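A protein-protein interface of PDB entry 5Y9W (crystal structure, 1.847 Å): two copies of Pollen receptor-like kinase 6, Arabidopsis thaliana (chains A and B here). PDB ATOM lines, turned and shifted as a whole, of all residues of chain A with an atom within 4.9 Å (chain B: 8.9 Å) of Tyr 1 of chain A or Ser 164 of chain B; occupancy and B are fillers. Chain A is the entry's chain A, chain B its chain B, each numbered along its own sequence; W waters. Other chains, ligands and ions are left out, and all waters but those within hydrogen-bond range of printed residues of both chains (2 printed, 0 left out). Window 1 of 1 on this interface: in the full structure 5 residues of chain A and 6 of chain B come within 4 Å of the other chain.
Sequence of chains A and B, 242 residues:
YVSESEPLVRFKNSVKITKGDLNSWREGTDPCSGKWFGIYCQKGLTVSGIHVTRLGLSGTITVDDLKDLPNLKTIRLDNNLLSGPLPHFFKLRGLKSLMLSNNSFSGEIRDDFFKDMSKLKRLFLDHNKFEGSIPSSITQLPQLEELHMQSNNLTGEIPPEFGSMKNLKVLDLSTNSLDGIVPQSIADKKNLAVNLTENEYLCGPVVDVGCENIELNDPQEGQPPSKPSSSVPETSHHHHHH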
ATOM      1  N   TYR A   1      -6.680   3.639   0.367  1.00  0.00           N
ATOM      2  CA  TYR A   1      -5.668   3.465  -0.671  1.00  0.00           C
ATOM      3  C   TYR A   1      -6.179   4.005  -2.001  1.00  0.00           C
ATOM      4  O   TYR A   1      -7.366   3.921  -2.294  1.00  0.00           O
ATOM      5  CB  TYR A   1      -5.270   1.973  -0.788  1.00  0.00           C
ATOM      6  CG  TYR A   1      -4.590   1.422   0.460  1.00  0.00           C
ATOM      7  CD1 TYR A   1      -3.402   1.972   0.912  1.00  0.00           C
ATOM      8  CD2 TYR A   1      -5.142   0.369   1.186  1.00  0.00           C
ATOM      9  CE1 TYR A   1      -2.774   1.502   2.046  1.00  0.00           C
ATOM     10  CE2 TYR A   1      -4.514  -0.124   2.339  1.00  0.00           C
ATOM     11  CZ  TYR A   1      -3.323   0.460   2.749  1.00  0.00           C
ATOM     12  OH  TYR A   1      -2.661   0.011   3.852  1.00  0.00           O
ATOM     13  N   VAL A   2      -5.275   4.578  -2.802  1.00  0.00           N
ATOM     14  CA  VAL A   2      -5.652   5.139  -4.099  1.00  0.00           C
ATOM     15  C   VAL A   2      -6.365   4.109  -4.967  1.00  0.00           C
ATOM     16  O   VAL A   2      -7.255   4.457  -5.748  1.00  0.00           O
ATOM     17  CB  VAL A   2      -4.405   5.712  -4.809  1.00  0.00           C
ATOM     18  CG1 VAL A   2      -4.733   6.132  -6.231  1.00  0.00           C
ATOM     19  CG2 VAL A   2      -3.853   6.903  -4.032  1.00  0.00           C
ATOM     20  N   SER A   3      -6.021   2.827  -4.815  1.00  0.00           N
ATOM     21  CA  SER A   3      -6.656   1.781  -5.613  1.00  0.00           C
ATOM     22  C   SER A   3      -8.141   1.624  -5.300  1.00  0.00           C
ATOM     23  O   SER A   3      -8.856   0.961  -6.059  1.00  0.00           O
ATOM     24  CB  SER A   3      -5.952   0.445  -5.394  1.00  0.00           C
ATOM     25  OG  SER A   3      -6.294  -0.149  -4.137  1.00  0.00           O
ATOM     26  N   GLU A   4      -8.621   2.203  -4.202  1.00  0.00           N
ATOM     27  CA  GLU A   4     -10.032   2.104  -3.858  1.00  0.00           C
ATOM     28  C   GLU A   4     -10.863   3.250  -4.425  1.00  0.00           C
ATOM     29  O   GLU A   4     -12.096   3.167  -4.409  1.00  0.00           O
ATOM     30  CB  GLU A   4     -10.173   2.004  -2.331  1.00  0.00           C
ATOM     31  CG  GLU A   4      -9.588   0.665  -1.799  1.00  0.00           C
ATOM     32  CD  GLU A   4      -9.290   0.664  -0.316  1.00  0.00           C
ATOM     33  OE1 GLU A   4      -8.968   1.743   0.225  1.00  0.00           O
ATOM     34  OE2 GLU A   4      -9.367  -0.418   0.312  1.00  0.00           O
ATOM     35  N   SER A   5     -10.229   4.301  -4.957  1.00  0.00           N
ATOM     36  CA  SER A   5     -11.008   5.390  -5.541  1.00  0.00           C
ATOM     37  C   SER A   5     -11.718   4.952  -6.811  1.00  0.00           C
ATOM     38  O   SER A   5     -12.820   5.431  -7.103  1.00  0.00           O
ATOM     39  CB  SER A   5     -10.125   6.606  -5.829  1.00  0.00           C
ATOM     40  OG  SER A   5      -9.174   6.357  -6.844  1.00  0.00           O
ATOM     41  N   ASP A  30      -6.657   9.334  -2.721  1.00  0.00           N
ATOM     42  CA  ASP A  30      -6.942   8.302  -1.733  1.00  0.00           C
ATOM     43  C   ASP A  30      -8.249   8.612  -1.016  1.00  0.00           C
ATOM     44  O   ASP A  30      -8.366   9.677  -0.392  1.00  0.00           O
ATOM     45  CB  ASP A  30      -5.807   8.208  -0.722  1.00  0.00           C
ATOM     46  CG  ASP A  30      -5.794   6.883   0.026  1.00  0.00           C
ATOM     47  OD1 ASP A  30      -6.871   6.328   0.343  1.00  0.00           O
ATOM     48  OD2 ASP A  30      -4.688   6.391   0.305  1.00  0.00           O
ATOM     49  N   PRO A  31      -9.242   7.721  -1.061  1.00  0.00           N
ATOM     50  CA  PRO A  31     -10.490   7.977  -0.329  1.00  0.00           C
ATOM     51  C   PRO A  31     -10.329   7.954   1.185  1.00  0.00           C
ATOM     52  O   PRO A  31     -11.284   8.307   1.893  1.00  0.00           O
ATOM     53  CB  PRO A  31     -11.436   6.868  -0.815  1.00  0.00           C
ATOM     54  CG  PRO A  31     -10.574   5.858  -1.503  1.00  0.00           C
ATOM     55  CD  PRO A  31      -9.282   6.494  -1.880  1.00  0.00           C
ATOM     56  N   CYS A  32      -9.157   7.577   1.699  1.00  0.00           N
ATOM     57  CA  CYS A  32      -8.875   7.612   3.129  1.00  0.00           C
ATOM     58  C   CYS A  32      -8.048   8.839   3.519  1.00  0.00           C
ATOM     59  O   CYS A  32      -7.437   8.858   4.589  1.00  0.00           O
ATOM     60  CB  CYS A  32      -8.179   6.318   3.556  1.00  0.00           C
ATOM     61  SG  CYS A  32      -9.210   4.836   3.311  1.00  0.00           S
ATOM     62  N   GLN A  42     -10.481   1.961   7.743  1.00  0.00           N
ATOM     63  CA  GLN A  42      -9.896   1.253   8.852  1.00  0.00           C
ATOM     64  C   GLN A  42      -8.488   1.826   9.023  1.00  0.00           C
ATOM     65  O   GLN A  42      -7.688   1.772   8.142  1.00  0.00           O
ATOM     66  CB  GLN A  42      -9.811  -0.240   8.606  1.00  0.00           C
ATOM     67  CG  GLN A  42      -9.290  -1.003   9.778  1.00  0.00           C
ATOM     68  CD  GLN A  42      -8.782  -2.387   9.422  1.00  0.00           C
ATOM     69  OE1 GLN A  42      -7.886  -2.543   8.631  1.00  0.00           O
ATOM     70  NE2 GLN A  42      -9.364  -3.380  10.016  1.00  0.00           N
ATOM     71  N   LEU A  45      -6.436   3.925   6.539  1.00  0.00           N
ATOM     72  CA  LEU A  45      -5.737   3.323   5.420  1.00  0.00           C
ATOM     73  C   LEU A  45      -6.564   2.758   4.284  1.00  0.00           C
ATOM     74  O   LEU A  45      -6.278   3.022   3.177  1.00  0.00           O
ATOM     75  CB  LEU A  45      -4.709   2.295   5.907  1.00  0.00           C
ATOM     76  CG  LEU A  45      -3.534   2.744   6.783  1.00  0.00           C
ATOM     77  CD1 LEU A  45      -2.723   1.583   7.290  1.00  0.00           C
ATOM     78  CD2 LEU A  45      -2.676   3.665   6.035  1.00  0.00           C
ATOM     79  N   THR A  46      -7.568   1.973   4.597  1.00  0.00           N
ATOM     80  CA  THR A  46      -8.371   1.292   3.602  1.00  0.00           C
ATOM     81  C   THR A  46      -9.846   1.546   3.862  1.00  0.00           C
ATOM     82  O   THR A  46     -10.286   1.588   5.018  1.00  0.00           O
ATOM     83  CB  THR A  46      -8.066  -0.242   3.608  1.00  0.00           C
ATOM     84  OG1 THR A  46      -8.942  -0.922   2.704  1.00  0.00           O
ATOM     85  CG2 THR A  46      -8.247  -0.821   4.989  1.00  0.00           C
ATOM     86  N   THR B 139      -1.477  -9.485  -0.284  1.00  0.00           N
ATOM     87  CA  THR B 139      -1.886  -8.511   0.720  1.00  0.00           C
ATOM     88  C   THR B 139      -3.279  -8.779   1.275  1.00  0.00           C
ATOM     89  O   THR B 139      -3.670  -8.111   2.239  1.00  0.00           O
ATOM     90  CB  THR B 139      -1.854  -7.077   0.153  1.00  0.00           C
ATOM     91  OG1 THR B 139      -2.847  -6.936  -0.871  1.00  0.00           O
ATOM     92  CG2 THR B 139      -0.467  -6.733  -0.418  1.00  0.00           C
ATOM     93  N   GLN B 140      -4.034  -9.714   0.687  1.00  0.00           N
ATOM     94  CA  GLN B 140      -5.368 -10.080   1.152  1.00  0.00           C
ATOM     95  C   GLN B 140      -5.374 -11.303   2.069  1.00  0.00           C
ATOM     96  O   GLN B 140      -6.449 -11.779   2.454  1.00  0.00           O
ATOM     97  CB  GLN B 140      -6.268 -10.311  -0.053  1.00  0.00           C
ATOM     98  CG  GLN B 140      -6.320  -9.104  -0.957  1.00  0.00           C
ATOM     99  CD  GLN B 140      -6.746  -7.875  -0.188  1.00  0.00           C
ATOM    100  OE1 GLN B 140      -7.816  -7.880   0.439  1.00  0.00           O
ATOM    101  NE2 GLN B 140      -5.907  -6.815  -0.203  1.00  0.00           N
ATOM    102  N   LEU B 141      -4.210 -11.818   2.435  1.00  0.00           N
ATOM    103  CA  LEU B 141      -4.127 -12.970   3.322  1.00  0.00           C
ATOM    104  C   LEU B 141      -4.387 -12.550   4.763  1.00  0.00           C
ATOM    105  O   LEU B 141      -3.517 -11.942   5.404  1.00  0.00           O
ATOM    106  CB  LEU B 141      -2.754 -13.637   3.195  1.00  0.00           C
ATOM    107  CG  LEU B 141      -2.464 -14.307   1.853  1.00  0.00           C
ATOM    108  CD1 LEU B 141      -0.980 -14.669   1.732  1.00  0.00           C
ATOM    109  CD2 LEU B 141      -3.332 -15.557   1.713  1.00  0.00           C
ATOM    110  N   PRO B 142      -5.546 -12.914   5.323  1.00  0.00           N
ATOM    111  CA  PRO B 142      -5.947 -12.344   6.622  1.00  0.00           C
ATOM    112  C   PRO B 142      -5.044 -12.735   7.774  1.00  0.00           C
ATOM    113  O   PRO B 142      -4.965 -11.993   8.759  1.00  0.00           O
ATOM    114  CB  PRO B 142      -7.365 -12.897   6.831  1.00  0.00           C
ATOM    115  CG  PRO B 142      -7.774 -13.511   5.517  1.00  0.00           C
ATOM    116  CD  PRO B 142      -6.505 -13.912   4.825  1.00  0.00           C
ATOM    117  N   LEU B 144      -1.621 -13.698   7.531  1.00  0.00           N
ATOM    118  CA  LEU B 144      -0.196 -13.712   7.228  1.00  0.00           C
ATOM    119  C   LEU B 144       0.598 -12.935   8.276  1.00  0.00           C
ATOM    120  O   LEU B 144       0.296 -11.773   8.579  1.00  0.00           O
ATOM    121  CB  LEU B 144       0.037 -13.125   5.838  1.00  0.00           C
ATOM    122  CG  LEU B 144       1.450 -13.417   5.333  1.00  0.00           C
ATOM    123  CD1 LEU B 144       1.599 -14.915   5.047  1.00  0.00           C
ATOM    124  CD2 LEU B 144       1.763 -12.548   4.121  1.00  0.00           C
ATOM    125  N   ILE B 158       5.760  -1.496  -4.652  1.00  0.00           N
ATOM    126  CA  ILE B 158       5.312  -2.275  -3.501  1.00  0.00           C
ATOM    127  C   ILE B 158       3.860  -1.912  -3.209  1.00  0.00           C
ATOM    128  O   ILE B 158       3.550  -0.710  -3.056  1.00  0.00           O
ATOM    129  CB  ILE B 158       6.196  -1.981  -2.298  1.00  0.00           C
ATOM    130  CG1 ILE B 158       7.649  -2.374  -2.604  1.00  0.00           C
ATOM    131  CG2 ILE B 158       5.624  -2.689  -1.048  1.00  0.00           C
ATOM    132  CD1 ILE B 158       8.654  -1.929  -1.546  1.00  0.00           C
ATOM    133  N   PRO B 159       2.948  -2.877  -3.134  1.00  0.00           N
ATOM    134  CA  PRO B 159       1.539  -2.539  -2.855  1.00  0.00           C
ATOM    135  C   PRO B 159       1.389  -1.889  -1.491  1.00  0.00           C
ATOM    136  O   PRO B 159       1.872  -2.405  -0.470  1.00  0.00           O
ATOM    137  CB  PRO B 159       0.805  -3.893  -2.914  1.00  0.00           C
ATOM    138  CG  PRO B 159       1.841  -4.940  -3.133  1.00  0.00           C
ATOM    139  CD  PRO B 159       3.117  -4.284  -3.553  1.00  0.00           C
ATOM    140  N   PRO B 160       0.726  -0.735  -1.432  1.00  0.00           N
ATOM    141  CA  PRO B 160       0.498  -0.096  -0.128  1.00  0.00           C
ATOM    142  C   PRO B 160      -0.372  -0.923   0.802  1.00  0.00           C
ATOM    143  O   PRO B 160      -0.330  -0.710   2.018  1.00  0.00           O
ATOM    144  CB  PRO B 160      -0.179   1.240  -0.499  1.00  0.00           C
ATOM    145  CG  PRO B 160      -0.735   1.030  -1.876  1.00  0.00           C
ATOM    146  CD  PRO B 160       0.218   0.072  -2.563  1.00  0.00           C
ATOM    147  N   GLU B 161      -1.155  -1.862   0.268  1.00  0.00           N
ATOM    148  CA  GLU B 161      -2.049  -2.680   1.082  1.00  0.00           C
ATOM    149  C   GLU B 161      -1.313  -3.556   2.085  1.00  0.00           C
ATOM    150  O   GLU B 161      -1.965  -4.120   2.965  1.00  0.00           O
ATOM    151  CB  GLU B 161      -2.938  -3.544   0.179  1.00  0.00           C
ATOM    152  CG  GLU B 161      -3.930  -2.765  -0.684  1.00  0.00           C
ATOM    153  CD  GLU B 161      -3.309  -2.112  -1.908  1.00  0.00           C
ATOM    154  OE1 GLU B 161      -2.147  -2.413  -2.247  1.00  0.00           O
ATOM    155  OE2 GLU B 161      -3.994  -1.276  -2.546  1.00  0.00           O
ATOM    156  N   PHE B 162       0.021  -3.709   1.971  1.00  0.00           N
ATOM    157  CA  PHE B 162       0.774  -4.358   3.046  1.00  0.00           C
ATOM    158  C   PHE B 162       0.579  -3.661   4.393  1.00  0.00           C
ATOM    159  O   PHE B 162       0.621  -4.313   5.441  1.00  0.00           O
ATOM    160  CB  PHE B 162       2.261  -4.400   2.716  1.00  0.00           C
ATOM    161  CG  PHE B 162       2.651  -5.562   1.843  1.00  0.00           C
ATOM    162  CD1 PHE B 162       2.483  -6.868   2.289  1.00  0.00           C
ATOM    163  CD2 PHE B 162       3.188  -5.343   0.580  1.00  0.00           C
ATOM    164  CE1 PHE B 162       2.844  -7.961   1.473  1.00  0.00           C
ATOM    165  CE2 PHE B 162       3.563  -6.408  -0.245  1.00  0.00           C
ATOM    166  CZ  PHE B 162       3.392  -7.727   0.197  1.00  0.00           C
ATOM    167  N   GLY B 163       0.388  -2.339   4.392  1.00  0.00           N
ATOM    168  CA  GLY B 163       0.270  -1.614   5.644  1.00  0.00           C
ATOM    169  C   GLY B 163      -0.977  -1.920   6.438  1.00  0.00           C
ATOM    170  O   GLY B 163      -1.024  -1.614   7.630  1.00  0.00           O
ATOM    171  N   SER B 164      -1.992  -2.495   5.811  1.00  0.00           N
ATOM    172  CA  SER B 164      -3.230  -2.837   6.495  1.00  0.00           C
ATOM    173  C   SER B 164      -3.273  -4.283   6.975  1.00  0.00           C
ATOM    174  O   SER B 164      -4.294  -4.711   7.529  1.00  0.00           O
ATOM    175  CB  SER B 164      -4.423  -2.568   5.572  1.00  0.00           C
ATOM    176  OG  SER B 164      -4.616  -1.177   5.415  1.00  0.00           O
ATOM    177  N   MET B 165      -2.202  -5.049   6.800  1.00  0.00           N
ATOM    178  CA  MET B 165      -2.237  -6.459   7.183  1.00  0.00           C
ATOM    179  C   MET B 165      -2.038  -6.580   8.690  1.00  0.00           C
ATOM    180  O   MET B 165      -0.931  -6.392   9.206  1.00  0.00           O
ATOM    181  CB  MET B 165      -1.196  -7.247   6.391  1.00  0.00           C
ATOM    182  CG  MET B 165      -1.462  -7.183   4.891  1.00  0.00           C
ATOM    183  SD  MET B 165      -0.336  -8.277   3.998  1.00  0.00           S
ATOM    184  CE  MET B 165      -1.045  -9.873   4.424  1.00  0.00           C
ATOM    185  N   LYS B 166      -3.128  -6.920   9.384  1.00  0.00           N
ATOM    186  CA  LYS B 166      -3.193  -6.852  10.844  1.00  0.00           C
ATOM    187  C   LYS B 166      -2.102  -7.674  11.517  1.00  0.00           C
ATOM    188  O   LYS B 166      -1.507  -7.235  12.508  1.00  0.00           O
ATOM    189  CB  LYS B 166      -4.584  -7.325  11.293  1.00  0.00           C
ATOM    190  CG  LYS B 166      -4.791  -7.502  12.785  1.00  0.00           C
ATOM    191  CD  LYS B 166      -6.215  -8.004  13.091  1.00  0.00           C
ATOM    192  CE  LYS B 166      -6.512  -9.341  12.403  1.00  0.00           C
ATOM    193  NZ  LYS B 166      -6.572 -10.492  13.364  1.00  0.00           N
ATOM    194  N   ASN B 167      -1.825  -8.874  11.007  1.00  0.00           N
ATOM    195  CA  ASN B 167      -0.925  -9.790  11.692  1.00  0.00           C
ATOM    196  C   ASN B 167       0.499  -9.760  11.157  1.00  0.00           C
ATOM    197  O   ASN B 167       1.355 -10.472  11.685  1.00  0.00           O
ATOM    198  CB  ASN B 167      -1.481 -11.212  11.605  1.00  0.00           C
ATOM    199  CG  ASN B 167      -2.855 -11.309  12.214  1.00  0.00           C
ATOM    200  OD1 ASN B 167      -3.001 -11.120  13.414  1.00  0.00           O
ATOM    201  ND2 ASN B 167      -3.868 -11.555  11.394  1.00  0.00           N
ATOM    202  N   LEU B 168       0.783  -8.949  10.139  1.00  0.00           N
ATOM    203  CA  LEU B 168       2.090  -9.013   9.494  1.00  0.00           C
ATOM    204  C   LEU B 168       3.174  -8.407  10.387  1.00  0.00           C
ATOM    205  O   LEU B 168       3.117  -7.226  10.758  1.00  0.00           O
ATOM    206  CB  LEU B 168       2.030  -8.312   8.136  1.00  0.00           C
ATOM    207  CG  LEU B 168       3.306  -8.381   7.291  1.00  0.00           C
ATOM    208  CD1 LEU B 168       3.542  -9.785   6.714  1.00  0.00           C
ATOM    209  CD2 LEU B 168       3.218  -7.354   6.178  1.00  0.00           C
ATOM    210  N   PRO B 183       5.556   2.747   0.368  1.00  0.00           N
ATOM    211  CA  PRO B 183       4.271   3.222   0.904  1.00  0.00           C
ATOM    212  C   PRO B 183       4.413   3.718   2.334  1.00  0.00           C
ATOM    213  O   PRO B 183       5.004   3.056   3.185  1.00  0.00           O
ATOM    214  CB  PRO B 183       3.373   1.981   0.830  1.00  0.00           C
ATOM    215  CG  PRO B 183       3.952   1.164  -0.280  1.00  0.00           C
ATOM    216  CD  PRO B 183       5.443   1.408  -0.244  1.00  0.00           C
ATOM    217  N   GLN B 184       3.832   4.891   2.602  1.00  0.00           N
ATOM    218  CA  GLN B 184       3.825   5.401   3.967  1.00  0.00           C
ATOM    219  C   GLN B 184       3.169   4.420   4.931  1.00  0.00           C
ATOM    220  O   GLN B 184       3.555   4.352   6.102  1.00  0.00           O
ATOM    221  CB  GLN B 184       3.096   6.745   4.021  1.00  0.00           C
ATOM    222  CG  GLN B 184       3.303   7.493   5.334  1.00  0.00           C
ATOM    223  CD  GLN B 184       4.757   7.863   5.565  1.00  0.00           C
ATOM    224  OE1 GLN B 184       5.480   8.236   4.634  1.00  0.00           O
ATOM    225  NE2 GLN B 184       5.195   7.759   6.809  1.00  0.00           N
ATOM    226  N   SER B 185       2.160   3.672   4.460  1.00  0.00           N
ATOM    227  CA  SER B 185       1.489   2.699   5.322  1.00  0.00           C
ATOM    228  C   SER B 185       2.462   1.665   5.874  1.00  0.00           C
ATOM    229  O   SER B 185       2.270   1.160   6.983  1.00  0.00           O
ATOM    230  CB  SER B 185       0.379   1.996   4.547  1.00  0.00           C
ATOM    231  OG  SER B 185       0.941   1.203   3.496  1.00  0.00           O
ATOM    232  N   ILE B 186       3.505   1.333   5.113  1.00  0.00           N
ATOM    233  CA  ILE B 186       4.499   0.382   5.589  1.00  0.00           C
ATOM    234  C   ILE B 186       5.471   1.057   6.545  1.00  0.00           C
ATOM    235  O   ILE B 186       5.816   0.500   7.595  1.00  0.00           O
ATOM    236  CB  ILE B 186       5.218  -0.250   4.381  1.00  0.00           C
ATOM    237  CG1 ILE B 186       4.221  -1.101   3.602  1.00  0.00           C
ATOM    238  CG2 ILE B 186       6.420  -1.077   4.843  1.00  0.00           C
ATOM    239  CD1 ILE B 186       4.775  -1.623   2.274  1.00  0.00           C
ATOM    240  N   LYS B 189       3.905   1.310  10.034  1.00  0.00           N
ATOM    241  CA  LYS B 189       3.316   0.126  10.645  1.00  0.00           C
ATOM    242  C   LYS B 189       4.087  -0.247  11.908  1.00  0.00           C
ATOM    243  O   LYS B 189       5.308  -0.432  11.872  1.00  0.00           O
ATOM    244  CB  LYS B 189       3.316  -1.032   9.653  1.00  0.00           C
ATOM    245  CG  LYS B 189       2.552  -2.252  10.126  1.00  0.00           C
ATOM    246  CD  LYS B 189       2.097  -3.066   8.937  1.00  0.00           C
ATOM    247  CE  LYS B 189       1.834  -4.510   9.326  1.00  0.00           C
ATOM    248  NZ  LYS B 189       0.656  -4.699  10.212  1.00  0.00           N
ATOM    249  N   LEU B 192       6.635  -3.953  12.991  1.00  0.00           N
ATOM    250  CA  LEU B 192       6.986  -4.583  11.720  1.00  0.00           C
ATOM    251  C   LEU B 192       8.496  -4.558  11.550  1.00  0.00           C
ATOM    252  O   LEU B 192       9.118  -3.496  11.640  1.00  0.00           O
ATOM    253  CB  LEU B 192       6.338  -3.872  10.527  1.00  0.00           C
ATOM    254  CG  LEU B 192       6.630  -4.452   9.133  1.00  0.00           C
ATOM    255  CD1 LEU B 192       6.070  -5.873   9.020  1.00  0.00           C
ATOM    256  CD2 LEU B 192       5.995  -3.542   8.065  1.00  0.00           C
HETATM  257  O   HOH W   1      -3.335   1.788  -3.669  1.00  0.00           O
HETATM  258  O   HOH W   2      -5.857  -0.544   7.968  1.00  0.00           O
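The side-chain hydroxyl of Tyr 1 of chain A lies within hydrogen-bond range of the backbone carbonyl oxygen of Pro 160 of chain B (3.1 Å). OE2 of Glu 161 of chain B is in hydrogen-bond range of OG of Ser 3 of chain A, 3.0 Å away. OH of Tyr 1 of chain A sits at hydrogen-bond distance from OG of Ser 164 of chain B, at 2.8 Å.
OG of Ser 185 of chain B sits at hydrogen-bond distance from O of Pro 160 of chain B, 2.7 Å away. The backbone NH of Tyr 1 of chain A lies within hydrogen-bond range of the side-chain carboxylate of Glu 4 of chain A (3.0 Å). N of Tyr 1 of chain A sits at hydrogen-bond distance from OD1 of Asp 30 of chain A, at 2.7 Å. N of Tyr 1 of chain A lies within hydrogen-bond range of O of Leu 45 of chain A (2.9 Å). The side-chain carboxylate (OE2) of Glu 4 of chain A is in hydrogen-bond range of the side-chain hydroxyl (OG1) of Thr 46 of chain A. The backbone NH (N) of Thr 46 of chain A lies close to the side-chain sulfur (SG) of Cys 32 of chain A (3.5 Å).
Among the printed residues, pairs that only touch across the chains: Tyr 1 of chain A with Glu 161 of chain B (3.8 Å), Tyr 1 of chain A with Gly 163 of chain B (3.6 Å), Tyr 1 of chain A with Ser 185 of chain B (3.7 Å), Leu 45 of chain A with Gly 163 of chain B (3.6 Å), Leu 45 of chain A with Ser 164 of chain B (3.5 Å), Leu 45 of chain A with Ser 185 of chain B (3.8 Å) and Thr 46 of chain A with Ser 164 of chain B (3.7 Å).
Printed residues of chain B within 4 Å of Ser 3 of chain A: Glu 161. Pro 31 of chain A touches none of the printed residues of chain B. Pro 142 of chain B touches none of the printed residues of chain A. Of the printed residues of chain A, Glu 161 of chain B touches Tyr 1 and Ser 3. Ser 164 of chain B touches just these residues of chain A: Tyr 1 (2.8 Å), Leu 45 (3.5 Å) and Thr 46 (3.7 Å). Printed residues of chain A within 4 Å of Ser 185 of chain B: Tyr 1 (3.7 Å) and Leu 45 (3.8 Å). The nearest residue of chain A that does not touch Ser 164 of chain B is Gln 42 of chain A (4.3 Å).
Of the 22 printed residues of chain B, 5 touch a printed residue of chain A. Printed residues of chain B that touch a printed residue of chain A: Pro 160, Glu 161, Gly 163, Ser 164 and Ser 185. Hydrophobic or aromatic side chains of chain B that line the printed part of chain A: Pro 160. Of the 11 printed residues of chain A, 4 touch a printed residue of chain B. Hydrophobic or aromatic side chains of chain A that line the printed part of chain B: Tyr 1 and Leu 45. Among the printed residues, 10 pairs touch across the chains. Among the printed residues, no Asp or Glu carboxylate lies within 4 Å of a Lys or Arg side-chain nitrogen of the other chain.
No position is printed for both chains.
Water W2 lies within hydrogen-bond range of the side-chain hydroxyl (OG) of Ser 164 of chain B (2.9 Å) and the side-chain amide oxygen (OE1) of Gln 42 of chain A (2.9 Å). Water W1 bridges N of Ser 3 of chain A (3.1 Å) and OE2 of Glu 161 of chain B (3.3 Å).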
